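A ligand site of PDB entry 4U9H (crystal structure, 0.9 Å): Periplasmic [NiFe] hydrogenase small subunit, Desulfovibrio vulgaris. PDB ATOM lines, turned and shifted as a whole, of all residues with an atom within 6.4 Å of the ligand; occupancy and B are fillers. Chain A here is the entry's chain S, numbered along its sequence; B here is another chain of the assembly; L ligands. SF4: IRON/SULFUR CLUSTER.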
ATOM      1  N   ALA A  13      25.646  -0.771  -8.000  1.00  0.00           N
ATOM      2  CA  ALA A  13      24.439   0.084  -7.978  1.00  0.00           C
ATOM      3  C   ALA A  13      23.552  -0.416  -9.127  1.00  0.00           C
ATOM      4  O   ALA A  13      23.798  -0.139 -10.293  1.00  0.00           O
ATOM      5  CB  ALA A  13      24.804   1.544  -8.155  1.00  0.00           C
ATOM      6  N   GLU A  14      22.535  -1.194  -8.742  1.00  0.00           N
ATOM      7  CA  GLU A  14      21.756  -1.987  -9.680  1.00  0.00           C
ATOM      8  C   GLU A  14      20.351  -2.137  -9.154  1.00  0.00           C
ATOM      9  O   GLU A  14      20.066  -1.929  -7.973  1.00  0.00           O
ATOM     10  CB  GLU A  14      22.421  -3.361  -9.968  1.00  0.00           C
ATOM     11  CG  GLU A  14      22.921  -4.111  -8.757  1.00  0.00           C
ATOM     12  CD  GLU A  14      21.914  -4.881  -7.963  1.00  0.00           C
ATOM     13  OE1 GLU A  14      21.046  -5.493  -8.602  1.00  0.00           O
ATOM     14  OE2 GLU A  14      22.035  -4.922  -6.702  1.00  0.00           O
ATOM     15  N   CYS A  15      19.447  -2.546 -10.057  1.00  0.00           N
ATOM     16  CA  CYS A  15      18.069  -2.795  -9.753  1.00  0.00           C
ATOM     17  C   CYS A  15      17.720  -4.271  -9.685  1.00  0.00           C
ATOM     18  O   CYS A  15      16.574  -4.632  -9.365  1.00  0.00           O
ATOM     19  CB  CYS A  15      17.126  -2.085 -10.738  1.00  0.00           C
ATOM     20  SG  CYS A  15      16.928  -2.972 -12.327  1.00  0.00           S
ATOM     21  N   THR A  16      18.678  -5.128 -10.026  1.00  0.00           N
ATOM     22  CA  THR A  16      18.556  -6.588 -10.043  1.00  0.00           C
ATOM     23  C   THR A  16      17.783  -7.073 -11.276  1.00  0.00           C
ATOM     24  O   THR A  16      17.609  -8.302 -11.460  1.00  0.00           O
ATOM     25  CB  THR A  16      18.064  -7.136  -8.683  1.00  0.00           C
ATOM     26  OG1 THR A  16      18.796  -6.460  -7.651  1.00  0.00           O
ATOM     27  CG2 THR A  16      18.236  -8.625  -8.530  1.00  0.00           C
ATOM     28  N   GLY A  17      17.416  -6.176 -12.175  1.00  0.00           N
ATOM     29  CA  GLY A  17      16.812  -6.588 -13.433  1.00  0.00           C
ATOM     30  C   GLY A  17      17.753  -7.381 -14.309  1.00  0.00           C
ATOM     31  O   GLY A  17      17.335  -8.271 -15.040  1.00  0.00           O
ATOM     32  N   CYS A  18      19.046  -7.064 -14.248  1.00  0.00           N
ATOM     33  CA  CYS A  18      20.012  -7.854 -15.013  1.00  0.00           C
ATOM     34  C   CYS A  18      20.104  -9.258 -14.444  1.00  0.00           C
ATOM     35  O   CYS A  18      20.079 -10.241 -15.191  1.00  0.00           O
ATOM     36  CB  CYS A  18      21.355  -7.159 -15.067  1.00  0.00           C
ATOM     37  SG  CYS A  18      21.375  -5.701 -16.166  1.00  0.00           S
ATOM     38  N   SER A  19      20.162  -9.417 -13.114  1.00  0.00           N
ATOM     39  CA  SER A  19      20.147 -10.765 -12.528  1.00  0.00           C
ATOM     40  C   SER A  19      18.900 -11.518 -12.953  1.00  0.00           C
ATOM     41  O   SER A  19      18.969 -12.702 -13.284  1.00  0.00           O
ATOM     42  CB  SER A  19      20.167 -10.699 -10.995  1.00  0.00           C
ATOM     43  OG  SER A  19      21.420 -10.407 -10.451  1.00  0.00           O
ATOM     44  N   GLU A  73      27.129  -6.619 -12.396  1.00  0.00           N
ATOM     45  CA  GLU A  73      25.880  -5.914 -12.598  1.00  0.00           C
ATOM     46  C   GLU A  73      25.923  -4.615 -11.779  1.00  0.00           C
ATOM     47  O   GLU A  73      26.283  -4.647 -10.610  1.00  0.00           O
ATOM     48  CB  GLU A  73      24.719  -6.807 -12.125  1.00  0.00           C
ATOM     49  CG  GLU A  73      23.318  -6.207 -12.127  1.00  0.00           C
ATOM     50  CD  GLU A  73      22.216  -7.213 -11.780  1.00  0.00           C
ATOM     51  OE1 GLU A  73      22.583  -8.360 -11.479  1.00  0.00           O
ATOM     52  OE2 GLU A  73      21.029  -6.839 -11.853  1.00  0.00           O
ATOM     53  N   GLY A  74      25.514  -3.517 -12.400  1.00  0.00           N
ATOM     54  CA  GLY A  74      25.410  -2.247 -11.714  1.00  0.00           C
ATOM     55  C   GLY A  74      26.611  -1.334 -11.948  1.00  0.00           C
ATOM     56  O   GLY A  74      27.739  -1.760 -12.189  1.00  0.00           O
ATOM     57  N   GLY A  75      26.322  -0.021 -11.851  1.00  0.00           N
ATOM     58  CA  GLY A  75      27.359   0.972 -11.900  1.00  0.00           C
ATOM     59  C   GLY A  75      28.114   1.073 -10.584  1.00  0.00           C
ATOM     60  O   GLY A  75      27.635   0.642  -9.537  1.00  0.00           O
ATOM     61  N   TYR A 109      27.688  -6.610 -17.340  1.00  0.00           N
ATOM     62  CA  TYR A 109      26.382  -7.061 -17.817  1.00  0.00           C
ATOM     63  C   TYR A 109      25.337  -6.010 -17.439  1.00  0.00           C
ATOM     64  O   TYR A 109      25.098  -5.784 -16.248  1.00  0.00           O
ATOM     65  CB  TYR A 109      26.062  -8.430 -17.252  1.00  0.00           C
ATOM     66  CG  TYR A 109      24.793  -9.030 -17.826  1.00  0.00           C
ATOM     67  CD1 TYR A 109      24.664  -9.286 -19.190  1.00  0.00           C
ATOM     68  CD2 TYR A 109      23.701  -9.333 -17.028  1.00  0.00           C
ATOM     69  CE1 TYR A 109      23.510  -9.793 -19.743  1.00  0.00           C
ATOM     70  CE2 TYR A 109      22.537  -9.836 -17.543  1.00  0.00           C
ATOM     71  CZ  TYR A 109      22.421 -10.064 -18.927  1.00  0.00           C
ATOM     72  OH  TYR A 109      21.285 -10.558 -19.509  1.00  0.00           O
ATOM     73  N   GLY A 110      24.750  -5.404 -18.459  1.00  0.00           N
ATOM     74  CA  GLY A 110      23.761  -4.350 -18.337  1.00  0.00           C
ATOM     75  C   GLY A 110      24.354  -2.973 -18.535  1.00  0.00           C
ATOM     76  O   GLY A 110      25.511  -2.728 -18.190  1.00  0.00           O
ATOM     77  N   THR A 111      23.536  -2.072 -19.069  1.00  0.00           N
ATOM     78  CA  THR A 111      23.947  -0.696 -19.317  1.00  0.00           C
ATOM     79  C   THR A 111      24.514   0.002 -18.093  1.00  0.00           C
ATOM     80  O   THR A 111      25.410   0.829 -18.225  1.00  0.00           O
ATOM     81  CB  THR A 111      22.782   0.063 -19.972  1.00  0.00           C
ATOM     82  OG1 THR A 111      22.606  -0.559 -21.243  1.00  0.00           O
ATOM     83  CG2 THR A 111      23.049   1.550 -20.138  1.00  0.00           C
ATOM     84  N   CYS A 112      24.040  -0.312 -16.882  1.00  0.00           N
ATOM     85  CA  CYS A 112      24.657   0.274 -15.693  1.00  0.00           C
ATOM     86  C   CYS A 112      26.139  -0.123 -15.578  1.00  0.00           C
ATOM     87  O   CYS A 112      27.006   0.730 -15.407  1.00  0.00           O
ATOM     88  CB  CYS A 112      23.933  -0.110 -14.428  1.00  0.00           C
ATOM     89  SG  CYS A 112      22.229   0.532 -14.310  1.00  0.00           S
ATOM     90  N   ALA A 113      26.428  -1.416 -15.604  1.00  0.00           N
ATOM     91  CA  ALA A 113      27.800  -1.883 -15.522  1.00  0.00           C
ATOM     92  C   ALA A 113      28.626  -1.461 -16.721  1.00  0.00           C
ATOM     93  O   ALA A 113      29.826  -1.194 -16.597  1.00  0.00           O
ATOM     94  CB  ALA A 113      27.835  -3.372 -15.334  1.00  0.00           C
ATOM     95  N   GLY A 117      24.627   3.820 -16.542  1.00  0.00           N
ATOM     96  CA  GLY A 117      23.217   3.517 -16.387  1.00  0.00           C
ATOM     97  C   GLY A 117      22.414   4.562 -15.648  1.00  0.00           C
ATOM     98  O   GLY A 117      22.732   5.756 -15.619  1.00  0.00           O
ATOM     99  N   VAL A 118      21.306   4.102 -15.056  1.00  0.00           N
ATOM    100  CA  VAL A 118      20.244   5.020 -14.625  1.00  0.00           C
ATOM    101  C   VAL A 118      20.745   5.968 -13.533  1.00  0.00           C
ATOM    102  O   VAL A 118      20.441   7.155 -13.550  1.00  0.00           O
ATOM    103  CB  VAL A 118      18.984   4.241 -14.224  1.00  0.00           C
ATOM    104  CG1 VAL A 118      19.172   3.401 -12.964  1.00  0.00           C
ATOM    105  CG2 VAL A 118      17.785   5.180 -14.106  1.00  0.00           C
ATOM    106  N   GLN A 119      21.546   5.457 -12.590  1.00  0.00           N
ATOM    107  CA  GLN A 119      22.046   6.324 -11.499  1.00  0.00           C
ATOM    108  C   GLN A 119      23.109   7.303 -11.999  1.00  0.00           C
ATOM    109  O   GLN A 119      23.402   8.263 -11.311  1.00  0.00           O
ATOM    110  CB  GLN A 119      22.562   5.506 -10.318  1.00  0.00           C
ATOM    111  CG  GLN A 119      23.630   4.471 -10.628  1.00  0.00           C
ATOM    112  CD  GLN A 119      23.052   3.157 -11.092  1.00  0.00           C
ATOM    113  OE1 GLN A 119      22.084   2.670 -10.520  1.00  0.00           O
ATOM    114  NE2 GLN A 119      23.619   2.587 -12.152  1.00  0.00           N
ATOM    115  N   GLY A 147      22.265  -3.101 -22.518  1.00  0.00           N
ATOM    116  CA  GLY A 147      20.820  -3.244 -22.496  1.00  0.00           C
ATOM    117  C   GLY A 147      20.337  -3.093 -21.039  1.00  0.00           C
ATOM    118  O   GLY A 147      21.098  -3.282 -20.094  1.00  0.00           O
ATOM    119  N   CYS A 148      19.038  -2.791 -20.894  1.00  0.00           N
ATOM    120  CA  CYS A 148      18.493  -2.414 -19.586  1.00  0.00           C
ATOM    121  C   CYS A 148      17.180  -3.176 -19.317  1.00  0.00           C
ATOM    122  O   CYS A 148      16.086  -2.584 -19.253  1.00  0.00           O
ATOM    123  CB  CYS A 148      18.306  -0.903 -19.515  1.00  0.00           C
ATOM    124  SG  CYS A 148      18.055  -0.224 -17.848  1.00  0.00           S
ATOM    125  N   PRO A 149      17.255  -4.490 -19.097  1.00  0.00           N
ATOM    126  CA  PRO A 149      18.473  -5.304 -19.111  1.00  0.00           C
ATOM    127  C   PRO A 149      18.783  -5.836 -20.497  1.00  0.00           C
ATOM    128  O   PRO A 149      17.956  -5.783 -21.434  1.00  0.00           O
ATOM    129  CB  PRO A 149      18.105  -6.463 -18.166  1.00  0.00           C
ATOM    130  CG  PRO A 149      16.614  -6.656 -18.422  1.00  0.00           C
ATOM    131  CD  PRO A 149      16.082  -5.243 -18.645  1.00  0.00           C
ATOM    132  N   PRO A 150      19.992  -6.387 -20.669  1.00  0.00           N
ATOM    133  CA  PRO A 150      20.323  -7.034 -21.942  1.00  0.00           C
ATOM    134  C   PRO A 150      19.484  -8.266 -22.185  1.00  0.00           C
ATOM    135  O   PRO A 150      18.834  -8.830 -21.285  1.00  0.00           O
ATOM    136  CB  PRO A 150      21.800  -7.465 -21.772  1.00  0.00           C
ATOM    137  CG  PRO A 150      22.278  -6.638 -20.588  1.00  0.00           C
ATOM    138  CD  PRO A 150      21.063  -6.561 -19.692  1.00  0.00           C
ATOM    139  N   TRP A 256      19.785   7.597 -21.006  1.00  0.00           N
ATOM    140  CA  TRP A 256      18.862   8.334 -20.180  1.00  0.00           C
ATOM    141  C   TRP A 256      18.864   9.830 -20.494  1.00  0.00           C
ATOM    142  O   TRP A 256      17.847  10.489 -20.385  1.00  0.00           O
ATOM    143  CB  TRP A 256      19.214   8.099 -18.696  1.00  0.00           C
ATOM    144  CG  TRP A 256      19.100   6.659 -18.315  1.00  0.00           C
ATOM    145  CD1 TRP A 256      20.102   5.756 -18.127  1.00  0.00           C
ATOM    146  CD2 TRP A 256      17.873   5.943 -18.133  1.00  0.00           C
ATOM    147  NE1 TRP A 256      19.589   4.524 -17.820  1.00  0.00           N
ATOM    148  CE2 TRP A 256      18.226   4.614 -17.813  1.00  0.00           C
ATOM    149  CE3 TRP A 256      16.522   6.290 -18.216  1.00  0.00           C
ATOM    150  CZ2 TRP A 256      17.271   3.629 -17.596  1.00  0.00           C
ATOM    151  CZ3 TRP A 256      15.576   5.313 -18.008  1.00  0.00           C
ATOM    152  CH2 TRP A 256      15.940   3.990 -17.707  1.00  0.00           C
ATOM    153  N   ARG B  40      20.911   5.471  -4.870  1.00  0.00           N
ATOM    154  CA  ARG B  40      21.026   5.856  -6.273  1.00  0.00           C
ATOM    155  C   ARG B  40      20.501   7.279  -6.537  1.00  0.00           C
ATOM    156  O   ARG B  40      21.100   8.011  -7.335  1.00  0.00           O
ATOM    157  CB  ARG B  40      20.330   4.843  -7.182  1.00  0.00           C
ATOM    158  CG  ARG B  40      21.094   3.525  -7.261  1.00  0.00           C
ATOM    159  CD  ARG B  40      20.363   2.445  -8.057  1.00  0.00           C
ATOM    160  NE  ARG B  40      19.136   2.067  -7.361  1.00  0.00           N
ATOM    161  CZ  ARG B  40      18.043   1.605  -7.934  1.00  0.00           C
ATOM    162  NH1 ARG B  40      18.021   1.289  -9.219  1.00  0.00           N
ATOM    163  NH2 ARG B  40      16.921   1.538  -7.214  1.00  0.00           N
ATOM    164  N   ARG B  60      13.213   1.311 -13.371  1.00  0.00           N
ATOM    165  CA  ARG B  60      14.551   0.883 -12.979  1.00  0.00           C
ATOM    166  C   ARG B  60      14.838   1.080 -11.501  1.00  0.00           C
ATOM    167  O   ARG B  60      15.938   0.800 -11.047  1.00  0.00           O
ATOM    168  CB  ARG B  60      15.629   1.507 -13.850  1.00  0.00           C
ATOM    169  CG  ARG B  60      15.786   0.882 -15.226  1.00  0.00           C
ATOM    170  CD  ARG B  60      14.558   0.935 -16.086  1.00  0.00           C
ATOM    171  NE  ARG B  60      14.887   0.460 -17.422  1.00  0.00           N
ATOM    172  CZ  ARG B  60      14.025   0.360 -18.402  1.00  0.00           C
ATOM    173  NH1 ARG B  60      12.840   0.983 -18.305  1.00  0.00           N
ATOM    174  NH2 ARG B  60      14.333  -0.366 -19.473  1.00  0.00           N
ATOM    175  N   CYS B  62      13.600  -1.071  -9.646  1.00  0.00           N
ATOM    176  CA  CYS B  62      13.683  -2.495  -9.265  1.00  0.00           C
ATOM    177  C   CYS B  62      13.288  -3.363 -10.442  1.00  0.00           C
ATOM    178  O   CYS B  62      12.242  -3.166 -11.059  1.00  0.00           O
ATOM    179  CB  CYS B  62      12.752  -2.754  -8.103  1.00  0.00           C
ATOM    180  SG  CYS B  62      12.963  -4.439  -7.436  1.00  0.00           S
ATOM    181  N   GLY B  63      14.140  -4.372 -10.690  1.00  0.00           N
ATOM    182  CA  GLY B  63      13.874  -5.377 -11.710  1.00  0.00           C
ATOM    183  C   GLY B  63      13.343  -6.706 -11.177  1.00  0.00           C
ATOM    184  O   GLY B  63      13.053  -7.577 -11.990  1.00  0.00           O
ATOM    185  N   PRO B 215      12.734  -8.887 -17.962  1.00  0.00           N
ATOM    186  CA  PRO B 215      12.336  -7.735 -17.154  1.00  0.00           C
ATOM    187  C   PRO B 215      12.151  -6.449 -17.955  1.00  0.00           C
ATOM    188  O   PRO B 215      12.679  -6.258 -19.053  1.00  0.00           O
ATOM    189  CB  PRO B 215      13.508  -7.548 -16.150  1.00  0.00           C
ATOM    190  CG  PRO B 215      14.190  -8.925 -16.141  1.00  0.00           C
ATOM    191  CD  PRO B 215      14.058  -9.402 -17.552  1.00  0.00           C
ATOM    192  N   HIS B 216      11.439  -5.539 -17.300  1.00  0.00           N
ATOM    193  CA  HIS B 216      11.230  -4.121 -17.653  1.00  0.00           C
ATOM    194  C   HIS B 216      10.327  -4.029 -18.866  1.00  0.00           C
ATOM    195  O   HIS B 216      10.745  -3.943 -20.024  1.00  0.00           O
ATOM    196  CB  HIS B 216      12.529  -3.336 -17.772  1.00  0.00           C
ATOM    197  CG  HIS B 216      13.209  -3.153 -16.444  1.00  0.00           C
ATOM    198  ND1 HIS B 216      12.532  -3.244 -15.232  1.00  0.00           N
ATOM    199  CD2 HIS B 216      14.513  -2.830 -16.193  1.00  0.00           C
ATOM    200  CE1 HIS B 216      13.425  -2.961 -14.286  1.00  0.00           C
ATOM    201  NE2 HIS B 216      14.621  -2.702 -14.830  1.00  0.00           N
HETATM  202 FE1  SF4 L   1      18.657  -2.480 -13.733  1.00  0.00          FE
HETATM  203 FE2  SF4 L   1      20.912  -1.312 -14.540  1.00  0.00          FE
HETATM  204 FE3  SF4 L   1      18.933  -1.624 -16.266  1.00  0.00          FE
HETATM  205 FE4  SF4 L   1      20.313  -3.843 -15.419  1.00  0.00          FE
HETATM  206  S1  SF4 L   1      21.147  -2.167 -16.692  1.00  0.00           S
HETATM  207  S2  SF4 L   1      18.019  -3.625 -15.676  1.00  0.00           S
HETATM  208  S3  SF4 L   1      20.840  -3.175 -13.230  1.00  0.00           S
HETATM  209  S4  SF4 L   1      18.850  -0.320 -14.313  1.00  0.00           S
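The backbone carbonyl oxygen (O) of Gly 147 sits close to a sulfur (S1) of the ligand, at 3.6 Å.
The backbone nitrogen (N) of Pro 149 lies close to a sulfur (S2) of the ligand (3.6 Å).
Residues that only touch the ligand: Glu 14 (3.6 Å), Gly 17 (3.9 Å), Glu 73 (3.9 Å), Gly 110 (3.8 Å), Val 118 (3.97 Å) and Arg 60 of chain B (3.4 Å).
Hydrophobic or aromatic side chains that line the ligand: Val 118, Pro 149 and His 216 of chain B.
14 residues have an atom within 4 Å of the ligand: Glu 14, Cys 15, Gly 17, Cys 18, Glu 73, Gly 110, Thr 111, Cys 112, Val 118, Gly 147, Cys 148, Pro 149, Arg 60 of chain B and His 216 of chain B.
The side-chain hydroxyl (OG) of Ser 19 lies within hydrogen-bond range of the side-chain carboxylate (OE1) of Glu 73, 2.6 Å away.
SG of Cys 15 lies close to NE2 of His 216 of chain B, at 3.4 Å.
The side-chain carboxylate of Glu 73 sits close to the backbone NH of Thr 16.
The backbone NH (N) of Val 118 lies close to the side-chain sulfur (SG) of Cys 112 (3.8 Å).
The backbone carbonyl oxygen (O) of Cys 15 is in hydrogen-bond range of the backbone NH (N) of Gly 63 of chain B (2.8 Å).
SG of Cys 18 sits close to O of Tyr 109 (3.7 Å).
The backbone carbonyl oxygen (O) of Cys 148 lies within hydrogen-bond range of the guanidinium group (NH2) of Arg 60 of chain B.
N of Cys 18 sits at hydrogen-bond distance from OE2 of Glu 73.
An iron atom (FE2) of the ligand is bound by the side-chain sulfur (SG) of Cys 112.
The side-chain sulfur (SG) of Cys 148 is bound to an iron atom (FE3) of the ligand (2.3 Å).
S2 of the ligand sits close to NE2 of His 216 of chain B (3.6 Å).
A sulfur (S3) of the ligand sits close to the backbone NH (N) of Cys 15, at 3.5 Å.
A sulfur (S1) of the ligand lies close to the backbone NH of Thr 111.
An iron atom (FE1) of the ligand is bound by the side-chain sulfur (SG) of Cys 15 (2.3 Å).
The backbone NH of Cys 112 lies close to a sulfur (S1) of the ligand, at 3.4 Å.
The side-chain sulfur of Cys 18 is bound to an iron atom (FE4) of the ligand, at 2.3 Å.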
